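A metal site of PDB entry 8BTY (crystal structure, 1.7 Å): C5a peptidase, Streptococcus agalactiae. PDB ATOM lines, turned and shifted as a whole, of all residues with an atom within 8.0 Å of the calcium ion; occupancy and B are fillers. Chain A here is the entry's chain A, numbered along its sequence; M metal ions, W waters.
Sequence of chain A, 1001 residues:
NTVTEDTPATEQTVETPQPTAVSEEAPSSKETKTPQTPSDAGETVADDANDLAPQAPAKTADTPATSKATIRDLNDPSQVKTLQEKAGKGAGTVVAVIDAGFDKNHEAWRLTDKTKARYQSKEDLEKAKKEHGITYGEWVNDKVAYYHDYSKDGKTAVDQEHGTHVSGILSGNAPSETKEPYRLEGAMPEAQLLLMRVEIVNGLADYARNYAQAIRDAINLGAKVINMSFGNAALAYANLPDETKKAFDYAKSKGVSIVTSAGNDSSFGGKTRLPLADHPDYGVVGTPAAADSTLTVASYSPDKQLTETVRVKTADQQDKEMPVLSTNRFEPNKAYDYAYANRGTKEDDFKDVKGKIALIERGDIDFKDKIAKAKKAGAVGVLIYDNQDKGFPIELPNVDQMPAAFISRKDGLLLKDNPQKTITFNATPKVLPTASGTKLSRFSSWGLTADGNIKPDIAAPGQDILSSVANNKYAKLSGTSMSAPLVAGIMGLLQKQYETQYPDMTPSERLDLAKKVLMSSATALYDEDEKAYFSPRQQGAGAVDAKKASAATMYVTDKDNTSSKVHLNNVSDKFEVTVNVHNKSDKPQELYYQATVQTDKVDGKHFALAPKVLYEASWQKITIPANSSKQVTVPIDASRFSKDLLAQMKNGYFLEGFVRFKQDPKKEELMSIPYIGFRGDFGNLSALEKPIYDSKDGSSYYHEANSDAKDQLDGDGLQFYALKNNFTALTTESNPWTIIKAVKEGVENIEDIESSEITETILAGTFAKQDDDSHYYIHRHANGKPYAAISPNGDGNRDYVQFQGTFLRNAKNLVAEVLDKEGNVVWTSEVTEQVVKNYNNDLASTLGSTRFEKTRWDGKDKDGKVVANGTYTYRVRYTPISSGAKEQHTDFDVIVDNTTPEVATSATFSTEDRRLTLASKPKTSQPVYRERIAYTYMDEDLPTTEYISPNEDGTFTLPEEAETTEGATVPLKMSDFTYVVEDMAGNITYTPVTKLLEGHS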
ATOM      1  N   GLU A 733       8.361  -4.114   9.968  1.00  0.00           N
ATOM      2  CA  GLU A 733       7.210  -4.480  10.782  1.00  0.00           C
ATOM      3  C   GLU A 733       5.924  -3.972  10.154  1.00  0.00           C
ATOM      4  O   GLU A 733       5.894  -2.867   9.590  1.00  0.00           O
ATOM      5  CB  GLU A 733       7.347  -3.956  12.228  1.00  0.00           C
ATOM      6  CG  GLU A 733       8.380  -4.734  13.033  1.00  0.00           C
ATOM      7  CD  GLU A 733       8.580  -4.212  14.428  1.00  0.00           C
ATOM      8  OE1 GLU A 733       7.574  -3.824  15.080  1.00  0.00           O
ATOM      9  OE2 GLU A 733       9.743  -4.197  14.874  1.00  0.00           O
ATOM     10  N   ASN A 735       2.251  -2.780  11.082  1.00  0.00           N
ATOM     11  CA  ASN A 735       1.454  -2.289  12.204  1.00  0.00           C
ATOM     12  C   ASN A 735       0.092  -1.901  11.674  1.00  0.00           C
ATOM     13  O   ASN A 735      -0.014  -0.902  10.929  1.00  0.00           O
ATOM     14  CB  ASN A 735       2.135  -1.103  12.901  1.00  0.00           C
ATOM     15  CG  ASN A 735       1.742  -0.991  14.371  1.00  0.00           C
ATOM     16  OD1 ASN A 735       1.272  -1.955  14.969  1.00  0.00           O
ATOM     17  ND2 ASN A 735       1.945   0.181  14.956  1.00  0.00           N
ATOM     18  N   ILE A 740      -2.104   1.434  15.353  1.00  0.00           N
ATOM     19  CA  ILE A 740      -1.646   2.809  15.166  1.00  0.00           C
ATOM     20  C   ILE A 740      -2.581   3.782  15.873  1.00  0.00           C
ATOM     21  O   ILE A 740      -2.143   4.659  16.634  1.00  0.00           O
ATOM     22  CB  ILE A 740      -1.528   3.138  13.661  1.00  0.00           C
ATOM     23  CG1 ILE A 740      -0.502   2.231  12.971  1.00  0.00           C
ATOM     24  CG2 ILE A 740      -1.191   4.638  13.474  1.00  0.00           C
ATOM     25  CD1 ILE A 740      -0.381   2.453  11.450  1.00  0.00           C
ATOM     26  N   ALA A 789      10.246  -0.806   0.856  1.00  0.00           N
ATOM     27  CA  ALA A 789       9.872   0.602   0.964  1.00  0.00           C
ATOM     28  C   ALA A 789       9.515   0.899   2.419  1.00  0.00           C
ATOM     29  O   ALA A 789       8.886   0.063   3.083  1.00  0.00           O
ATOM     30  CB  ALA A 789       8.694   0.957   0.059  1.00  0.00           C
ATOM     31  N   ILE A 790       9.917   2.074   2.902  1.00  0.00           N
ATOM     32  CA  ILE A 790       9.639   2.442   4.274  1.00  0.00           C
ATOM     33  C   ILE A 790       9.039   3.845   4.313  1.00  0.00           C
ATOM     34  O   ILE A 790       9.292   4.671   3.441  1.00  0.00           O
ATOM     35  CB  ILE A 790      10.879   2.389   5.192  1.00  0.00           C
ATOM     36  CG1 ILE A 790      11.990   3.298   4.647  1.00  0.00           C
ATOM     37  CG2 ILE A 790      11.337   0.935   5.380  1.00  0.00           C
ATOM     38  CD1 ILE A 790      13.130   3.527   5.658  1.00  0.00           C
ATOM     39  N   SER A 791       8.249   4.081   5.361  1.00  0.00           N
ATOM     40  CA  SER A 791       7.571   5.355   5.605  1.00  0.00           C
ATOM     41  C   SER A 791       8.024   5.798   6.988  1.00  0.00           C
ATOM     42  O   SER A 791       7.341   5.514   7.987  1.00  0.00           O
ATOM     43  CB  SER A 791       6.059   5.195   5.532  1.00  0.00           C
ATOM     44  OG  SER A 791       5.645   4.072   6.304  1.00  0.00           O
ATOM     45  N   PRO A 792       9.159   6.484   7.098  1.00  0.00           N
ATOM     46  CA  PRO A 792       9.735   6.806   8.416  1.00  0.00           C
ATOM     47  C   PRO A 792       8.999   7.966   9.088  1.00  0.00           C
ATOM     48  O   PRO A 792       9.454   9.099   9.162  1.00  0.00           O
ATOM     49  CB  PRO A 792      11.181   7.156   8.072  1.00  0.00           C
ATOM     50  CG  PRO A 792      11.072   7.766   6.701  1.00  0.00           C
ATOM     51  CD  PRO A 792      10.003   6.962   5.986  1.00  0.00           C
ATOM     52  N   ASN A 793       7.807   7.653   9.590  1.00  0.00           N
ATOM     53  CA  ASN A 793       6.966   8.630  10.275  1.00  0.00           C
ATOM     54  C   ASN A 793       6.626   8.198  11.690  1.00  0.00           C
ATOM     55  O   ASN A 793       5.727   8.770  12.305  1.00  0.00           O
ATOM     56  CB  ASN A 793       5.688   8.883   9.469  1.00  0.00           C
ATOM     57  CG  ASN A 793       4.949   7.591   9.119  1.00  0.00           C
ATOM     58  OD1 ASN A 793       5.183   6.548   9.745  1.00  0.00           O
ATOM     59  ND2 ASN A 793       4.061   7.663   8.131  1.00  0.00           N
ATOM     60  N   GLY A 794       7.308   7.187  12.220  1.00  0.00           N
ATOM     61  CA  GLY A 794       7.179   6.840  13.625  1.00  0.00           C
ATOM     62  C   GLY A 794       5.913   6.130  14.043  1.00  0.00           C
ATOM     63  O   GLY A 794       5.631   6.078  15.232  1.00  0.00           O
ATOM     64  N   ASP A 795       5.128   5.580  13.100  1.00  0.00           N
ATOM     65  CA  ASP A 795       3.921   4.868  13.517  1.00  0.00           C
ATOM     66  C   ASP A 795       4.124   3.364  13.669  1.00  0.00           C
ATOM     67  O   ASP A 795       3.163   2.653  14.001  1.00  0.00           O
ATOM     68  CB  ASP A 795       2.744   5.152  12.574  1.00  0.00           C
ATOM     69  CG  ASP A 795       2.969   4.671  11.142  1.00  0.00           C
ATOM     70  OD1 ASP A 795       4.005   4.028  10.816  1.00  0.00           O
ATOM     71  OD2 ASP A 795       2.082   4.966  10.316  1.00  0.00           O
ATOM     72  N   GLY A 796       5.342   2.863  13.478  1.00  0.00           N
ATOM     73  CA  GLY A 796       5.590   1.449  13.607  1.00  0.00           C
ATOM     74  C   GLY A 796       5.210   0.616  12.406  1.00  0.00           C
ATOM     75  O   GLY A 796       5.502  -0.594  12.385  1.00  0.00           O
ATOM     76  N   ASN A 797       4.578   1.213  11.399  1.00  0.00           N
ATOM     77  CA  ASN A 797       4.179   0.509  10.180  1.00  0.00           C
ATOM     78  C   ASN A 797       5.253   0.755   9.127  1.00  0.00           C
ATOM     79  O   ASN A 797       5.327   1.842   8.545  1.00  0.00           O
ATOM     80  CB  ASN A 797       2.807   0.968   9.682  1.00  0.00           C
ATOM     81  CG  ASN A 797       2.264   0.083   8.565  1.00  0.00           C
ATOM     82  OD1 ASN A 797       2.290  -1.142   8.664  1.00  0.00           O
ATOM     83  ND2 ASN A 797       1.800   0.714   7.486  1.00  0.00           N
ATOM     84  N   ARG A 798       6.091  -0.262   8.889  1.00  0.00           N
ATOM     85  CA  ARG A 798       7.105  -0.216   7.834  1.00  0.00           C
ATOM     86  C   ARG A 798       7.999   1.016   7.962  1.00  0.00           C
ATOM     87  O   ARG A 798       8.291   1.713   6.991  1.00  0.00           O
ATOM     88  CB  ARG A 798       6.443  -0.295   6.447  1.00  0.00           C
ATOM     89  CG  ARG A 798       5.657  -1.602   6.218  1.00  0.00           C
ATOM     90  CD  ARG A 798       4.811  -1.595   4.944  1.00  0.00           C
ATOM     91  NE  ARG A 798       4.053  -2.839   4.801  1.00  0.00           N
ATOM     92  CZ  ARG A 798       4.465  -3.900   4.124  1.00  0.00           C
ATOM     93  NH1 ARG A 798       5.599  -3.885   3.442  1.00  0.00           N
ATOM     94  NH2 ARG A 798       3.726  -5.014   4.139  1.00  0.00           N
ATOM     95  N   ASP A 799       8.441   1.297   9.196  1.00  0.00           N
ATOM     96  CA  ASP A 799       9.283   2.463   9.458  1.00  0.00           C
ATOM     97  C   ASP A 799      10.756   2.210   9.168  1.00  0.00           C
ATOM     98  O   ASP A 799      11.508   3.176   9.021  1.00  0.00           O
ATOM     99  CB  ASP A 799       9.186   2.892  10.932  1.00  0.00           C
ATOM    100  CG  ASP A 799       7.831   3.481  11.315  1.00  0.00           C
ATOM    101  OD1 ASP A 799       6.965   3.706  10.438  1.00  0.00           O
ATOM    102  OD2 ASP A 799       7.653   3.745  12.521  1.00  0.00           O
ATOM    103  N   TYR A 800      11.187   0.947   9.091  1.00  0.00           N
ATOM    104  CA  TYR A 800      12.610   0.656   9.050  1.00  0.00           C
ATOM    105  C   TYR A 800      12.857  -0.609   8.231  1.00  0.00           C
ATOM    106  O   TYR A 800      11.936  -1.375   7.959  1.00  0.00           O
ATOM    107  CB  TYR A 800      13.198   0.464  10.464  1.00  0.00           C
ATOM    108  CG  TYR A 800      12.756  -0.812  11.175  1.00  0.00           C
ATOM    109  CD1 TYR A 800      13.380  -2.035  10.922  1.00  0.00           C
ATOM    110  CD2 TYR A 800      11.745  -0.787  12.141  1.00  0.00           C
ATOM    111  CE1 TYR A 800      12.996  -3.198  11.565  1.00  0.00           C
ATOM    112  CE2 TYR A 800      11.354  -1.954  12.796  1.00  0.00           C
ATOM    113  CZ  TYR A 800      11.995  -3.150  12.512  1.00  0.00           C
ATOM    114  OH  TYR A 800      11.627  -4.329  13.149  1.00  0.00           O
ATOM    115  N   ASP A 897       9.547   6.859   1.431  1.00  0.00           N
ATOM    116  CA  ASP A 897       8.469   7.746   1.015  1.00  0.00           C
ATOM    117  C   ASP A 897       7.560   8.012   2.206  1.00  0.00           C
ATOM    118  O   ASP A 897       6.955   7.070   2.737  1.00  0.00           O
ATOM    119  CB  ASP A 897       7.674   7.160  -0.147  1.00  0.00           C
ATOM    120  CG  ASP A 897       6.826   8.187  -0.850  1.00  0.00           C
ATOM    121  OD1 ASP A 897       6.113   8.967  -0.173  1.00  0.00           O
ATOM    122  OD2 ASP A 897       6.865   8.221  -2.097  1.00  0.00           O
ATOM    123  N   ASN A 898       7.457   9.261   2.616  1.00  0.00           N
ATOM    124  CA  ASN A 898       6.626   9.615   3.767  1.00  0.00           C
ATOM    125  C   ASN A 898       5.381  10.411   3.366  1.00  0.00           C
ATOM    126  O   ASN A 898       4.803  11.094   4.216  1.00  0.00           O
ATOM    127  CB  ASN A 898       7.442  10.386   4.800  1.00  0.00           C
ATOM    128  CG  ASN A 898       7.921  11.744   4.299  1.00  0.00           C
ATOM    129  OD1 ASN A 898       7.644  12.151   3.172  1.00  0.00           O
ATOM    130  ND2 ASN A 898       8.654  12.458   5.159  1.00  0.00           N
ATOM    131  N   GLU A 982      -3.822   2.527   2.393  1.00  0.00           N
ATOM    132  CA  GLU A 982      -2.412   2.324   2.707  1.00  0.00           C
ATOM    133  C   GLU A 982      -1.640   2.183   1.404  1.00  0.00           C
ATOM    134  O   GLU A 982      -2.087   1.485   0.488  1.00  0.00           O
ATOM    135  CB  GLU A 982      -2.234   1.069   3.585  1.00  0.00           C
ATOM    136  CG  GLU A 982      -0.827   0.812   4.109  1.00  0.00           C
ATOM    137  CD  GLU A 982      -0.730  -0.474   4.929  1.00  0.00           C
ATOM    138  OE1 GLU A 982      -1.696  -1.265   4.914  1.00  0.00           O
ATOM    139  OE2 GLU A 982       0.322  -0.700   5.584  1.00  0.00           O
ATOM    140  N   ALA A 985       4.621   1.977   0.751  1.00  0.00           N
ATOM    141  CA  ALA A 985       5.620   2.290   1.760  1.00  0.00           C
ATOM    142  C   ALA A 985       5.065   2.194   3.184  1.00  0.00           C
ATOM    143  O   ALA A 985       5.818   2.394   4.146  1.00  0.00           O
ATOM    144  CB  ALA A 985       6.195   3.696   1.549  1.00  0.00           C
ATOM    145  N   GLY A 986       3.777   1.904   3.331  1.00  0.00           N
ATOM    146  CA  GLY A 986       3.147   1.886   4.640  1.00  0.00           C
ATOM    147  C   GLY A 986       2.491   3.189   5.063  1.00  0.00           C
ATOM    148  O   GLY A 986       1.958   3.256   6.177  1.00  0.00           O
ATOM    149  N   ASN A 987       2.519   4.220   4.225  1.00  0.00           N
ATOM    150  CA  ASN A 987       1.767   5.438   4.560  1.00  0.00           C
ATOM    151  C   ASN A 987       0.287   5.091   4.584  1.00  0.00           C
ATOM    152  O   ASN A 987      -0.196   4.316   3.754  1.00  0.00           O
ATOM    153  CB  ASN A 987       2.058   6.547   3.541  1.00  0.00           C
ATOM    154  CG  ASN A 987       3.497   6.977   3.562  1.00  0.00           C
ATOM    155  OD1 ASN A 987       3.942   7.608   4.527  1.00  0.00           O
ATOM    156  ND2 ASN A 987       4.255   6.629   2.519  1.00  0.00           N
ATOM    157  N   ILE A 988      -0.436   5.656   5.554  1.00  0.00           N
ATOM    158  CA  ILE A 988      -1.765   5.127   5.847  1.00  0.00           C
ATOM    159  C   ILE A 988      -2.659   6.236   6.376  1.00  0.00           C
ATOM    160  O   ILE A 988      -2.221   7.140   7.095  1.00  0.00           O
ATOM    161  CB  ILE A 988      -1.701   3.943   6.837  1.00  0.00           C
ATOM    162  CG1 ILE A 988      -3.054   3.234   6.906  1.00  0.00           C
ATOM    163  CG2 ILE A 988      -1.208   4.414   8.229  1.00  0.00           C
ATOM    164  CD1 ILE A 988      -2.988   1.862   7.587  1.00  0.00           C
HETATM  165 CA    CA M   1       5.422   4.227   8.835  1.00  0.00          CA
HETATM  166  O   HOH W   1       3.297   4.790   8.033  1.00  0.00           O
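Water W1 lies within hydrogen-bond range of OD2 of Asp 795 (2.6 Å), O of Gly 986 (2.8 Å) and ND2 of Asn 793 (3.0 Å).
OD2 of Asp 799 is in hydrogen-bond range of N of Gly 796, at 2.7 Å. The backbone NH (N) of Gly 794 sits close to the side-chain carboxylate (OD2) of Asp 799 (3.5 Å). ND2 of Asn 797 sits at hydrogen-bond distance from O of Gly 986, at 2.9 Å. The side-chain amide oxygen of Asn 797 sits at hydrogen-bond distance from the backbone NH of Asn 735 (2.9 Å). ND2 of Asn 797 lies within hydrogen-bond range of OE2 of Glu 982. The backbone carbonyl oxygen (O) of Asp 795 is in hydrogen-bond range of the side-chain amide nitrogen (ND2) of Asn 735, at 2.9 Å. The backbone NH (N) of Ser 791 lies within hydrogen-bond range of the backbone carbonyl oxygen (O) of Arg 798 (2.9 Å). The backbone NH of Ser 791 sits close to the backbone carbonyl oxygen of Ala 985 (3.2 Å).
Five residues have an atom within 4 Å of the calcium ion: Ser 791, Asn 793, Asp 795, Asn 797 and Asp 799. The nearest printed residue that does not touch the calcium ion is Arg 798 (4.2 Å).
The calcium ion is bound by OD1 of Asp 799 (2.3 Å), water W1 (2.3 Å), O of Asn 797 (2.4 Å), OD1 of Asp 795 (2.4 Å), O of Ser 791 (2.5 Å), OD1 of Asn 793 (2.5 Å) and OG of Ser 791 (2.5 Å). The calcium ion has seven donor atoms within binding distance.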
